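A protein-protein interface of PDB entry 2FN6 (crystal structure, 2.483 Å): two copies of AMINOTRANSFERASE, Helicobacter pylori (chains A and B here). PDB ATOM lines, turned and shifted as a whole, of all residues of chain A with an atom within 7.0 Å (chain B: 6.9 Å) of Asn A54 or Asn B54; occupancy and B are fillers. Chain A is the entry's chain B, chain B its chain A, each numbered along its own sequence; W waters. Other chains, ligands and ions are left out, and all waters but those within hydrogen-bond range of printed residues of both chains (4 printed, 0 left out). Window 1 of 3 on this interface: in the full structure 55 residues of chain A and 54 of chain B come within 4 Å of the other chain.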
ATOM      1  N   VAL A  52      -0.868 -17.328  22.554  1.00  0.00           N
ATOM      2  CA  VAL A  52      -0.910 -18.793  22.385  1.00  0.00           C
ATOM      3  C   VAL A  52      -0.938 -19.568  23.705  1.00  0.00           C
ATOM      4  O   VAL A  52      -0.299 -19.180  24.682  1.00  0.00           O
ATOM      5  CB  VAL A  52       0.200 -19.287  21.443  1.00  0.00           C
ATOM      6  CG1 VAL A  52      -0.003 -18.657  20.059  1.00  0.00           C
ATOM      7  CG2 VAL A  52       1.618 -18.988  22.034  1.00  0.00           C
ATOM      8  N   PHE A  53      -1.690 -20.664  23.713  1.00  0.00           N
ATOM      9  CA  PHE A  53      -1.969 -21.476  24.921  1.00  0.00           C
ATOM     10  C   PHE A  53      -1.694 -22.958  24.622  1.00  0.00           C
ATOM     11  O   PHE A  53      -1.591 -23.350  23.448  1.00  0.00           O
ATOM     12  CB  PHE A  53      -3.458 -21.340  25.311  1.00  0.00           C
ATOM     13  CG  PHE A  53      -3.860 -19.965  25.756  1.00  0.00           C
ATOM     14  CD1 PHE A  53      -3.957 -19.662  27.110  1.00  0.00           C
ATOM     15  CD2 PHE A  53      -4.125 -18.964  24.826  1.00  0.00           C
ATOM     16  CE1 PHE A  53      -4.317 -18.374  27.533  1.00  0.00           C
ATOM     17  CE2 PHE A  53      -4.485 -17.690  25.226  1.00  0.00           C
ATOM     18  CZ  PHE A  53      -4.578 -17.383  26.579  1.00  0.00           C
ATOM     19  N   ASN A  54      -1.625 -23.784  25.675  1.00  0.00           N
ATOM     20  CA  ASN A  54      -1.436 -25.225  25.537  1.00  0.00           C
ATOM     21  C   ASN A  54      -2.533 -25.904  24.733  1.00  0.00           C
ATOM     22  O   ASN A  54      -2.285 -26.922  24.109  1.00  0.00           O
ATOM     23  CB  ASN A  54      -1.325 -25.905  26.914  1.00  0.00           C
ATOM     24  CG  ASN A  54      -2.656 -25.904  27.691  1.00  0.00           C
ATOM     25  OD1 ASN A  54      -3.424 -26.874  27.657  1.00  0.00           O
ATOM     26  ND2 ASN A  54      -2.934 -24.809  28.365  1.00  0.00           N
ATOM     27  N   SER A  55      -3.748 -25.356  24.770  1.00  0.00           N
ATOM     28  CA  SER A  55      -4.883 -25.918  24.029  1.00  0.00           C
ATOM     29  C   SER A  55      -5.950 -24.851  23.806  1.00  0.00           C
ATOM     30  O   SER A  55      -5.930 -23.821  24.461  1.00  0.00           O
ATOM     31  CB  SER A  55      -5.487 -27.114  24.776  1.00  0.00           C
ATOM     32  OG  SER A  55      -6.158 -26.695  25.960  1.00  0.00           O
ATOM     33  N   ALA A  56      -6.879 -25.086  22.881  1.00  0.00           N
ATOM     34  CA  ALA A  56      -7.975 -24.132  22.665  1.00  0.00           C
ATOM     35  C   ALA A  56      -8.974 -24.091  23.828  1.00  0.00           C
ATOM     36  O   ALA A  56      -9.690 -23.109  24.016  1.00  0.00           O
ATOM     37  CB  ALA A  56      -8.690 -24.404  21.364  1.00  0.00           C
ATOM     38  N   THR A  57      -9.017 -25.158  24.611  1.00  0.00           N
ATOM     39  CA  THR A  57      -9.865 -25.176  25.776  1.00  0.00           C
ATOM     40  C   THR A  57      -9.345 -24.191  26.837  1.00  0.00           C
ATOM     41  O   THR A  57     -10.108 -23.397  27.361  1.00  0.00           O
ATOM     42  CB  THR A  57     -10.031 -26.615  26.278  1.00  0.00           C
ATOM     43  OG1 THR A  57     -10.547 -27.405  25.194  1.00  0.00           O
ATOM     44  CG2 THR A  57     -11.007 -26.680  27.455  1.00  0.00           C
ATOM     45  N   SER A  58      -8.044 -24.204  27.099  1.00  0.00           N
ATOM     46  CA  SER A  58      -7.438 -23.217  27.986  1.00  0.00           C
ATOM     47  C   SER A  58      -7.602 -21.777  27.502  1.00  0.00           C
ATOM     48  O   SER A  58      -7.731 -20.848  28.315  1.00  0.00           O
ATOM     49  CB  SER A  58      -5.964 -23.517  28.159  1.00  0.00           C
ATOM     50  OG  SER A  58      -5.797 -24.869  28.515  1.00  0.00           O
ATOM     51  N   ALA A  59      -7.583 -21.591  26.188  1.00  0.00           N
ATOM     52  CA  ALA A  59      -7.754 -20.268  25.598  1.00  0.00           C
ATOM     53  C   ALA A  59      -9.166 -19.792  25.861  1.00  0.00           C
ATOM     54  O   ALA A  59      -9.364 -18.637  26.220  1.00  0.00           O
ATOM     55  CB  ALA A  59      -7.466 -20.295  24.096  1.00  0.00           C
ATOM     56  N   THR A 187       0.037 -27.565  16.301  1.00  0.00           N
ATOM     57  CA  THR A 187       1.211 -27.577  17.159  1.00  0.00           C
ATOM     58  C   THR A 187       1.137 -28.835  18.056  1.00  0.00           C
ATOM     59  O   THR A 187       1.671 -28.849  19.166  1.00  0.00           O
ATOM     60  CB  THR A 187       1.326 -26.283  18.029  1.00  0.00           C
ATOM     61  OG1 THR A 187       0.332 -26.290  19.064  1.00  0.00           O
ATOM     62  CG2 THR A 187       1.172 -25.032  17.178  1.00  0.00           C
ATOM     63  N   ALA A 188       0.462 -29.871  17.544  1.00  0.00           N
ATOM     64  CA  ALA A 188       0.123 -31.110  18.276  1.00  0.00           C
ATOM     65  C   ALA A 188      -0.992 -30.890  19.309  1.00  0.00           C
ATOM     66  O   ALA A 188      -2.080 -31.484  19.210  1.00  0.00           O
ATOM     67  CB  ALA A 188       1.362 -31.765  18.903  1.00  0.00           C
ATOM     68  N   GLU A 189      -0.702 -30.054  20.298  1.00  0.00           N
ATOM     69  CA  GLU A 189      -1.715 -29.486  21.181  1.00  0.00           C
ATOM     70  C   GLU A 189      -1.457 -27.990  21.193  1.00  0.00           C
ATOM     71  O   GLU A 189      -0.298 -27.562  21.361  1.00  0.00           O
ATOM     72  CB  GLU A 189      -1.598 -30.017  22.627  1.00  0.00           C
ATOM     73  CG  GLU A 189      -2.032 -31.459  22.844  1.00  0.00           C
ATOM     74  CD  GLU A 189      -3.540 -31.656  22.863  1.00  0.00           C
ATOM     75  OE1 GLU A 189      -4.316 -30.683  22.711  1.00  0.00           O
ATOM     76  OE2 GLU A 189      -3.957 -32.812  23.032  1.00  0.00           O
ATOM     77  N   GLY A 190      -2.514 -27.203  21.003  1.00  0.00           N
ATOM     78  CA  GLY A 190      -2.400 -25.764  21.098  1.00  0.00           C
ATOM     79  C   GLY A 190      -3.624 -24.963  20.744  1.00  0.00           C
ATOM     80  O   GLY A 190      -4.529 -25.448  20.070  1.00  0.00           O
ATOM     81  N   GLY A 191      -3.618 -23.702  21.170  1.00  0.00           N
ATOM     82  CA  GLY A 191      -4.691 -22.769  20.830  1.00  0.00           C
ATOM     83  C   GLY A 191      -4.266 -21.318  20.912  1.00  0.00           C
ATOM     84  O   GLY A 191      -3.113 -20.998  21.266  1.00  0.00           O
ATOM     85  N   ARG A 208      -2.673 -16.501  31.832  1.00  0.00           N
ATOM     86  CA  ARG A 208      -1.962 -17.608  31.204  1.00  0.00           C
ATOM     87  C   ARG A 208      -0.723 -18.037  32.004  1.00  0.00           C
ATOM     88  O   ARG A 208      -0.253 -19.162  31.865  1.00  0.00           O
ATOM     89  CB  ARG A 208      -1.572 -17.227  29.779  1.00  0.00           C
ATOM     90  CG  ARG A 208      -0.984 -18.341  28.949  1.00  0.00           C
ATOM     91  CD  ARG A 208      -0.515 -17.810  27.595  1.00  0.00           C
ATOM     92  NE  ARG A 208       0.600 -16.861  27.688  1.00  0.00           N
ATOM     93  CZ  ARG A 208       1.179 -16.283  26.633  1.00  0.00           C
ATOM     94  NH1 ARG A 208       2.169 -15.434  26.816  1.00  0.00           N
ATOM     95  NH2 ARG A 208       0.774 -16.558  25.390  1.00  0.00           N
ATOM     96  N   ASN A 228      -0.986 -22.076  34.496  1.00  0.00           N
ATOM     97  CA  ASN A 228       0.120 -22.344  33.559  1.00  0.00           C
ATOM     98  C   ASN A 228      -0.412 -23.010  32.308  1.00  0.00           C
ATOM     99  O   ASN A 228      -0.458 -24.248  32.180  1.00  0.00           O
ATOM    100  CB  ASN A 228       1.281 -23.129  34.177  1.00  0.00           C
ATOM    101  CG  ASN A 228       2.411 -23.407  33.171  1.00  0.00           C
ATOM    102  OD1 ASN A 228       3.450 -24.001  33.518  1.00  0.00           O
ATOM    103  ND2 ASN A 228       2.205 -23.004  31.912  1.00  0.00           N
ATOM    104  N   PHE A 229      -0.835 -22.156  31.387  1.00  0.00           N
ATOM    105  CA  PHE A 229      -1.351 -22.603  30.112  1.00  0.00           C
ATOM    106  C   PHE A 229      -0.416 -22.208  28.973  1.00  0.00           C
ATOM    107  O   PHE A 229      -0.865 -22.078  27.843  1.00  0.00           O
ATOM    108  CB  PHE A 229      -2.726 -21.991  29.851  1.00  0.00           C
ATOM    109  CG  PHE A 229      -3.768 -22.347  30.870  1.00  0.00           C
ATOM    110  CD1 PHE A 229      -3.702 -23.539  31.584  1.00  0.00           C
ATOM    111  CD2 PHE A 229      -4.843 -21.499  31.089  1.00  0.00           C
ATOM    112  CE1 PHE A 229      -4.684 -23.865  32.525  1.00  0.00           C
ATOM    113  CE2 PHE A 229      -5.833 -21.814  32.015  1.00  0.00           C
ATOM    114  CZ  PHE A 229      -5.758 -23.011  32.725  1.00  0.00           C
ATOM    115  N   ARG A 230       0.869 -21.994  29.265  1.00  0.00           N
ATOM    116  CA  ARG A 230       1.819 -21.611  28.212  1.00  0.00           C
ATOM    117  C   ARG A 230       1.974 -22.683  27.116  1.00  0.00           C
ATOM    118  O   ARG A 230       1.794 -23.876  27.358  1.00  0.00           O
ATOM    119  CB  ARG A 230       3.185 -21.248  28.804  1.00  0.00           C
ATOM    120  CG  ARG A 230       3.165 -19.947  29.639  1.00  0.00           C
ATOM    121  CD  ARG A 230       4.529 -19.574  30.221  1.00  0.00           C
ATOM    122  NE  ARG A 230       5.191 -20.701  30.891  1.00  0.00           N
ATOM    123  CZ  ARG A 230       5.347 -20.846  32.208  1.00  0.00           C
ATOM    124  NH1 ARG A 230       4.885 -19.929  33.053  1.00  0.00           N
ATOM    125  NH2 ARG A 230       5.990 -21.911  32.678  1.00  0.00           N
ATOM    126  N   LEU A 231       2.263 -22.230  25.903  1.00  0.00           N
ATOM    127  CA  LEU A 231       2.671 -23.095  24.809  1.00  0.00           C
ATOM    128  C   LEU A 231       4.197 -23.040  24.858  1.00  0.00           C
ATOM    129  O   LEU A 231       4.774 -21.958  24.991  1.00  0.00           O
ATOM    130  CB  LEU A 231       2.134 -22.550  23.480  1.00  0.00           C
ATOM    131  CG  LEU A 231       2.188 -23.457  22.251  1.00  0.00           C
ATOM    132  CD1 LEU A 231       1.205 -24.650  22.354  1.00  0.00           C
ATOM    133  CD2 LEU A 231       1.921 -22.674  20.993  1.00  0.00           C
ATOM    134  N   ASN A 232       4.860 -24.189  24.793  1.00  0.00           N
ATOM    135  CA  ASN A 232       6.323 -24.204  24.844  1.00  0.00           C
ATOM    136  C   ASN A 232       6.979 -23.864  23.504  1.00  0.00           C
ATOM    137  O   ASN A 232       6.318 -23.758  22.465  1.00  0.00           O
ATOM    138  CB  ASN A 232       6.830 -25.554  25.344  1.00  0.00           C
ATOM    139  CG  ASN A 232       6.408 -26.679  24.457  1.00  0.00           C
ATOM    140  OD1 ASN A 232       5.544 -27.480  24.813  1.00  0.00           O
ATOM    141  ND2 ASN A 232       7.000 -26.752  23.287  1.00  0.00           N
ATOM    142  N   GLN A 235       6.526 -26.505  20.470  1.00  0.00           N
ATOM    143  CA  GLN A 235       5.305 -26.335  19.688  1.00  0.00           C
ATOM    144  C   GLN A 235       5.136 -24.978  18.993  1.00  0.00           C
ATOM    145  O   GLN A 235       4.448 -24.887  17.970  1.00  0.00           O
ATOM    146  CB  GLN A 235       4.037 -26.726  20.437  1.00  0.00           C
ATOM    147  CG  GLN A 235       4.163 -27.088  21.858  1.00  0.00           C
ATOM    148  CD  GLN A 235       3.272 -28.264  22.172  1.00  0.00           C
ATOM    149  OE1 GLN A 235       2.311 -28.156  22.943  1.00  0.00           O
ATOM    150  NE2 GLN A 235       3.560 -29.399  21.533  1.00  0.00           N
ATOM    151  N   VAL B  52      -0.303 -37.627  33.301  1.00  0.00           N
ATOM    152  CA  VAL B  52       0.535 -36.506  32.868  1.00  0.00           C
ATOM    153  C   VAL B  52      -0.276 -35.334  32.335  1.00  0.00           C
ATOM    154  O   VAL B  52      -1.265 -35.521  31.626  1.00  0.00           O
ATOM    155  CB  VAL B  52       1.601 -36.917  31.830  1.00  0.00           C
ATOM    156  CG1 VAL B  52       2.650 -37.834  32.465  1.00  0.00           C
ATOM    157  CG2 VAL B  52       0.944 -37.537  30.591  1.00  0.00           C
ATOM    158  N   PHE B  53       0.167 -34.123  32.667  1.00  0.00           N
ATOM    159  CA  PHE B  53      -0.556 -32.907  32.254  1.00  0.00           C
ATOM    160  C   PHE B  53       0.370 -31.953  31.507  1.00  0.00           C
ATOM    161  O   PHE B  53       1.600 -32.109  31.536  1.00  0.00           O
ATOM    162  CB  PHE B  53      -1.178 -32.184  33.473  1.00  0.00           C
ATOM    163  CG  PHE B  53      -2.148 -33.023  34.261  1.00  0.00           C
ATOM    164  CD1 PHE B  53      -3.516 -32.887  34.071  1.00  0.00           C
ATOM    165  CD2 PHE B  53      -1.694 -33.943  35.205  1.00  0.00           C
ATOM    166  CE1 PHE B  53      -4.422 -33.683  34.800  1.00  0.00           C
ATOM    167  CE2 PHE B  53      -2.594 -34.726  35.936  1.00  0.00           C
ATOM    168  CZ  PHE B  53      -3.957 -34.596  35.725  1.00  0.00           C
ATOM    169  N   ASN B  54      -0.217 -30.944  30.868  1.00  0.00           N
ATOM    170  CA  ASN B  54       0.557 -29.927  30.157  1.00  0.00           C
ATOM    171  C   ASN B  54       1.517 -29.156  31.068  1.00  0.00           C
ATOM    172  O   ASN B  54       2.570 -28.732  30.614  1.00  0.00           O
ATOM    173  CB  ASN B  54      -0.357 -28.971  29.405  1.00  0.00           C
ATOM    174  CG  ASN B  54      -1.099 -28.040  30.328  1.00  0.00           C
ATOM    175  OD1 ASN B  54      -0.692 -26.901  30.534  1.00  0.00           O
ATOM    176  ND2 ASN B  54      -2.186 -28.520  30.901  1.00  0.00           N
ATOM    177  N   SER B  55       1.147 -28.998  32.341  1.00  0.00           N
ATOM    178  CA  SER B  55       1.992 -28.364  33.363  1.00  0.00           C
ATOM    179  C   SER B  55       1.718 -28.963  34.752  1.00  0.00           C
ATOM    180  O   SER B  55       0.724 -29.653  34.942  1.00  0.00           O
ATOM    181  CB  SER B  55       1.767 -26.840  33.368  1.00  0.00           C
ATOM    182  OG  SER B  55       0.392 -26.488  33.558  1.00  0.00           O
ATOM    183  N   ALA B  56       2.599 -28.727  35.714  1.00  0.00           N
ATOM    184  CA  ALA B  56       2.341 -29.106  37.121  1.00  0.00           C
ATOM    185  C   ALA B  56       1.252 -28.251  37.756  1.00  0.00           C
ATOM    186  O   ALA B  56       0.492 -28.744  38.604  1.00  0.00           O
ATOM    187  CB  ALA B  56       3.613 -29.040  37.964  1.00  0.00           C
ATOM    188  N   THR B  57       1.159 -26.981  37.340  1.00  0.00           N
ATOM    189  CA  THR B  57       0.073 -26.116  37.773  1.00  0.00           C
ATOM    190  C   THR B  57      -1.305 -26.680  37.391  1.00  0.00           C
ATOM    191  O   THR B  57      -2.232 -26.637  38.187  1.00  0.00           O
ATOM    192  CB  THR B  57       0.238 -24.711  37.208  1.00  0.00           C
ATOM    193  OG1 THR B  57       1.500 -24.173  37.625  1.00  0.00           O
ATOM    194  CG2 THR B  57      -0.871 -23.811  37.684  1.00  0.00           C
ATOM    195  N   SER B  58      -1.430 -27.207  36.176  1.00  0.00           N
ATOM    196  CA  SER B  58      -2.661 -27.859  35.736  1.00  0.00           C
ATOM    197  C   SER B  58      -2.941 -29.145  36.523  1.00  0.00           C
ATOM    198  O   SER B  58      -4.086 -29.432  36.848  1.00  0.00           O
ATOM    199  CB  SER B  58      -2.593 -28.172  34.249  1.00  0.00           C
ATOM    200  OG  SER B  58      -2.489 -26.969  33.515  1.00  0.00           O
ATOM    201  N   ALA B  59      -1.880 -29.895  36.812  1.00  0.00           N
ATOM    202  CA  ALA B  59      -1.937 -31.100  37.636  1.00  0.00           C
ATOM    203  C   ALA B  59      -2.351 -30.797  39.091  1.00  0.00           C
ATOM    204  O   ALA B  59      -3.167 -31.521  39.658  1.00  0.00           O
ATOM    205  CB  ALA B  59      -0.585 -31.860  37.582  1.00  0.00           C
ATOM    206  N   THR B 187       9.894 -32.185  30.000  1.00  0.00           N
ATOM    207  CA  THR B 187       9.078 -32.365  28.798  1.00  0.00           C
ATOM    208  C   THR B 187       8.794 -30.986  28.173  1.00  0.00           C
ATOM    209  O   THR B 187       7.751 -30.782  27.513  1.00  0.00           O
ATOM    210  CB  THR B 187       7.707 -33.071  29.113  1.00  0.00           C
ATOM    211  OG1 THR B 187       6.945 -32.277  30.035  1.00  0.00           O
ATOM    212  CG2 THR B 187       7.907 -34.451  29.709  1.00  0.00           C
ATOM    213  N   ALA B 188       9.712 -30.044  28.406  1.00  0.00           N
ATOM    214  CA  ALA B 188       9.540 -28.617  28.062  1.00  0.00           C
ATOM    215  C   ALA B 188       8.546 -27.912  28.996  1.00  0.00           C
ATOM    216  O   ALA B 188       8.940 -27.018  29.744  1.00  0.00           O
ATOM    217  CB  ALA B 188       9.164 -28.415  26.580  1.00  0.00           C
ATOM    218  N   GLU B 189       7.269 -28.285  28.925  1.00  0.00           N
ATOM    219  CA  GLU B 189       6.289 -27.963  29.971  1.00  0.00           C
ATOM    220  C   GLU B 189       5.601 -29.282  30.244  1.00  0.00           C
ATOM    221  O   GLU B 189       5.462 -30.115  29.344  1.00  0.00           O
ATOM    222  CB  GLU B 189       5.230 -26.935  29.520  1.00  0.00           C
ATOM    223  CG  GLU B 189       5.738 -25.535  29.174  1.00  0.00           C
ATOM    224  CD  GLU B 189       5.851 -24.595  30.371  1.00  0.00           C
ATOM    225  OE1 GLU B 189       5.707 -25.051  31.522  1.00  0.00           O
ATOM    226  OE2 GLU B 189       6.091 -23.384  30.158  1.00  0.00           O
ATOM    227  N   GLY B 190       5.169 -29.494  31.478  1.00  0.00           N
ATOM    228  CA  GLY B 190       4.463 -30.724  31.780  1.00  0.00           C
ATOM    229  C   GLY B 190       4.482 -31.078  33.236  1.00  0.00           C
ATOM    230  O   GLY B 190       5.384 -30.689  33.968  1.00  0.00           O
ATOM    231  N   GLY B 191       3.471 -31.815  33.657  1.00  0.00           N
ATOM    232  CA  GLY B 191       3.446 -32.314  35.013  1.00  0.00           C
ATOM    233  C   GLY B 191       2.825 -33.683  35.120  1.00  0.00           C
ATOM    234  O   GLY B 191       2.457 -34.309  34.113  1.00  0.00           O
ATOM    235  N   ARG B 208      -9.073 -33.978  33.216  1.00  0.00           N
ATOM    236  CA  ARG B 208      -8.020 -33.723  32.242  1.00  0.00           C
ATOM    237  C   ARG B 208      -8.483 -33.608  30.794  1.00  0.00           C
ATOM    238  O   ARG B 208      -7.825 -32.944  29.981  1.00  0.00           O
ATOM    239  CB  ARG B 208      -6.955 -34.808  32.357  1.00  0.00           C
ATOM    240  CG  ARG B 208      -6.079 -34.927  31.149  1.00  0.00           C
ATOM    241  CD  ARG B 208      -4.664 -34.999  31.551  1.00  0.00           C
ATOM    242  NE  ARG B 208      -4.027 -36.316  31.498  1.00  0.00           N
ATOM    243  CZ  ARG B 208      -4.477 -37.421  30.915  1.00  0.00           C
ATOM    244  NH1 ARG B 208      -5.649 -37.467  30.301  1.00  0.00           N
ATOM    245  NH2 ARG B 208      -3.723 -38.502  30.965  1.00  0.00           N
ATOM    246  N   ASN B 228      -8.847 -29.348  28.669  1.00  0.00           N
ATOM    247  CA  ASN B 228      -7.845 -30.045  27.874  1.00  0.00           C
ATOM    248  C   ASN B 228      -6.516 -29.698  28.434  1.00  0.00           C
ATOM    249  O   ASN B 228      -5.927 -28.677  28.048  1.00  0.00           O
ATOM    250  CB  ASN B 228      -7.878 -29.690  26.385  1.00  0.00           C
ATOM    251  CG  ASN B 228      -6.844 -30.493  25.569  1.00  0.00           C
ATOM    252  OD1 ASN B 228      -6.874 -30.494  24.346  1.00  0.00           O
ATOM    253  ND2 ASN B 228      -5.939 -31.184  26.255  1.00  0.00           N
ATOM    254  N   PHE B 229      -6.063 -30.548  29.354  1.00  0.00           N
ATOM    255  CA  PHE B 229      -4.774 -30.411  30.002  1.00  0.00           C
ATOM    256  C   PHE B 229      -3.894 -31.588  29.627  1.00  0.00           C
ATOM    257  O   PHE B 229      -2.965 -31.944  30.377  1.00  0.00           O
ATOM    258  CB  PHE B 229      -4.903 -30.413  31.527  1.00  0.00           C
ATOM    259  CG  PHE B 229      -5.681 -29.269  32.094  1.00  0.00           C
ATOM    260  CD1 PHE B 229      -5.663 -28.013  31.499  1.00  0.00           C
ATOM    261  CD2 PHE B 229      -6.403 -29.440  33.274  1.00  0.00           C
ATOM    262  CE1 PHE B 229      -6.377 -26.966  32.054  1.00  0.00           C
ATOM    263  CE2 PHE B 229      -7.123 -28.387  33.839  1.00  0.00           C
ATOM    264  CZ  PHE B 229      -7.097 -27.153  33.231  1.00  0.00           C
ATOM    265  N   ARG B 230      -4.174 -32.212  28.488  1.00  0.00           N
ATOM    266  CA  ARG B 230      -3.369 -33.362  28.061  1.00  0.00           C
ATOM    267  C   ARG B 230      -1.907 -32.967  27.809  1.00  0.00           C
ATOM    268  O   ARG B 230      -1.592 -31.791  27.588  1.00  0.00           O
ATOM    269  CB  ARG B 230      -3.979 -34.043  26.829  1.00  0.00           C
ATOM    270  CG  ARG B 230      -5.426 -34.481  27.053  1.00  0.00           C
ATOM    271  CD  ARG B 230      -5.962 -35.363  25.934  1.00  0.00           C
ATOM    272  NE  ARG B 230      -6.009 -34.656  24.660  1.00  0.00           N
ATOM    273  CZ  ARG B 230      -7.064 -33.985  24.210  1.00  0.00           C
ATOM    274  NH1 ARG B 230      -8.178 -33.935  24.931  1.00  0.00           N
ATOM    275  NH2 ARG B 230      -7.001 -33.371  23.030  1.00  0.00           N
ATOM    276  N   LEU B 231      -1.023 -33.955  27.896  1.00  0.00           N
ATOM    277  CA  LEU B 231       0.350 -33.812  27.461  1.00  0.00           C
ATOM    278  C   LEU B 231       0.443 -34.537  26.126  1.00  0.00           C
ATOM    279  O   LEU B 231       0.052 -35.703  26.030  1.00  0.00           O
ATOM    280  CB  LEU B 231       1.322 -34.423  28.476  1.00  0.00           C
ATOM    281  CG  LEU B 231       2.810 -34.195  28.172  1.00  0.00           C
ATOM    282  CD1 LEU B 231       3.139 -32.684  28.206  1.00  0.00           C
ATOM    283  CD2 LEU B 231       3.718 -34.958  29.122  1.00  0.00           C
ATOM    284  N   ASN B 232       0.958 -33.857  25.101  1.00  0.00           N
ATOM    285  CA  ASN B 232       1.021 -34.439  23.767  1.00  0.00           C
ATOM    286  C   ASN B 232       2.163 -35.445  23.554  1.00  0.00           C
ATOM    287  O   ASN B 232       3.082 -35.549  24.368  1.00  0.00           O
ATOM    288  CB  ASN B 232       1.040 -33.342  22.708  1.00  0.00           C
ATOM    289  CG  ASN B 232       2.289 -32.489  22.767  1.00  0.00           C
ATOM    290  OD1 ASN B 232       2.205 -31.271  22.930  1.00  0.00           O
ATOM    291  ND2 ASN B 232       3.445 -33.113  22.642  1.00  0.00           N
ATOM    292  N   GLN B 235       5.939 -34.468  23.643  1.00  0.00           N
ATOM    293  CA  GLN B 235       6.465 -34.190  24.961  1.00  0.00           C
ATOM    294  C   GLN B 235       6.506 -35.451  25.815  1.00  0.00           C
ATOM    295  O   GLN B 235       7.380 -35.597  26.668  1.00  0.00           O
ATOM    296  CB  GLN B 235       5.689 -33.057  25.611  1.00  0.00           C
ATOM    297  CG  GLN B 235       6.002 -31.719  24.953  1.00  0.00           C
ATOM    298  CD  GLN B 235       5.073 -30.599  25.369  1.00  0.00           C
ATOM    299  OE1 GLN B 235       4.850 -30.351  26.558  1.00  0.00           O
ATOM    300  NE2 GLN B 235       4.538 -29.889  24.375  1.00  0.00           N
HETATM  301  O   HOH W   1      -2.147 -24.560  34.564  1.00  0.00           O
HETATM  302  O   HOH W   2      -2.758 -29.416  26.348  1.00  0.00           O
HETATM  303  O   HOH W   3      -7.953 -26.642  29.004  1.00  0.00           O
HETATM  304  O   HOH W   4       1.756 -25.245  29.706  1.00  0.00           O
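Among the printed residues, pairs that only touch across the chains: Phe A229 with Phe B229, Asn A228 with Thr B57, Asn A54 with Asn B54, Glu A189 with Asn B232, Thr A57 with Asn B228, Asn A228 with Ser B58, Ser A58 with Asn B228, Asn A232 with Ala B188, Phe A229 with Ser B58 and Asn A232 with Glu B189.
O of Asn A54 sits at hydrogen-bond distance from N of Gly A190 (3.1 Å). The side-chain amide nitrogen (ND2) of Asn B228 sits close to the backbone NH (N) of Arg B230 (3.0 Å). The side-chain hydroxyl of Ser A55 lies within hydrogen-bond range of the side-chain hydroxyl of Ser A58. O of Glu A189 lies within hydrogen-bond range of OG1 of Thr A187.
Ser A55 touches Asn B228, and with the chains exchanged Asn A228 touches Ser B55. Phe A229 touches Ser B58, but with the chains exchanged Ser A58 does not touch Phe B229 (4.2 Å). Asn A232 touches Gln B235, and with the chains exchanged Gln A235 touches Asn B232. Positions printed for both chains: 52, 53, 54, 55, 56, 57, 58, 59, 187, 188, 189, 190, 191, 208, 228, 229, 230, 231, 232 and 235.
Printed residues of chain B within 4 Å of Thr A57: Asn B228. Printed residues of chain B within 4 Å of Phe A229: Ser B58 (3.9 Å) and Phe B229 (3.6 Å). Of chain A, only Asn A54 (3.6 Å) and Asn A228 (3.1 Å) come within 4 Å of Asn B54. Of the printed residues of chain A, Gln B235 touches Asn A232 (2.6 Å) and Gln A235 (3.0 Å). The nearest residue of chain B that does not touch Asn A54 is Phe B229 (4.5 Å). The nearest residue of chain A that does not touch Asn B54 is Phe A229 (4.4 Å).
Water W1 lies within hydrogen-bond range of OG of Ser B58 (2.6 Å), N of Asn A228 (2.7 Å) and OG of Ser B55 (3.3 Å). Water W4 lies within hydrogen-bond range of O of Arg A230, OD1 of Asn B54 and ND2 of Asn A228. Water W3 lies within hydrogen-bond range of OG of Ser A58 and N of Asn B228. Water W2 bridges O of Arg B230 (2.9 Å) and OD1 of Asn A54 (2.9 Å).
The side-chain amide oxygen of Asn B54 lies close to the backbone carbonyl oxygen of Asn A228. NE2 of Gln B235 lies close to NE2 of Gln A235, 3.0 Å away. The guanidinium group (NH2) of Arg B230 is in salt-bridge range of the side-chain carboxylate (OE2) of Glu A189 (3.1 Å). The side-chain amide oxygen of Asn B228 lies close to the side-chain carboxylate of Glu A189, 3.0 Å away. The side-chain amide oxygen (OD1) of Asn A232 is in hydrogen-bond range of the side-chain amide nitrogen (NE2) of Gln B235 (2.6 Å). The side-chain hydroxyl (OG) of Ser B55 is in hydrogen-bond range of the backbone carbonyl oxygen (O) of Asn A228 (2.8 Å). NE2 of Gln A235 lies within hydrogen-bond range of OD1 of Asn B232 (2.7 Å). OD1 of Asn A228 sits close to OE1 of Glu B189, 3.2 Å away. O of Asn B228 lies within hydrogen-bond range of OG of Ser A55 (2.9 Å). The guanidinium group (NH2) of Arg A230 lies within salt-bridge range of the side-chain carboxylate (OE2) of Glu B189, 2.9 Å away. OD1 of Asn A54 lies close to O of Asn B228.
Of the 20 printed residues of chain A, 10 touch a printed residue of chain B. Hydrophobic or aromatic side chains of chain A that line the printed part of chain B: Phe A229. Along chain B the printed residues that touch a printed residue of chain A span positions 54 to 235. Among the printed residues, 21 pairs touch across the chains. Among the printed residues, Asp or Glu carboxylates within 4 Å of a Lys or Arg side-chain nitrogen of the other chain: Glu A189 with Arg B230 and Arg A230 with Glu B189.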
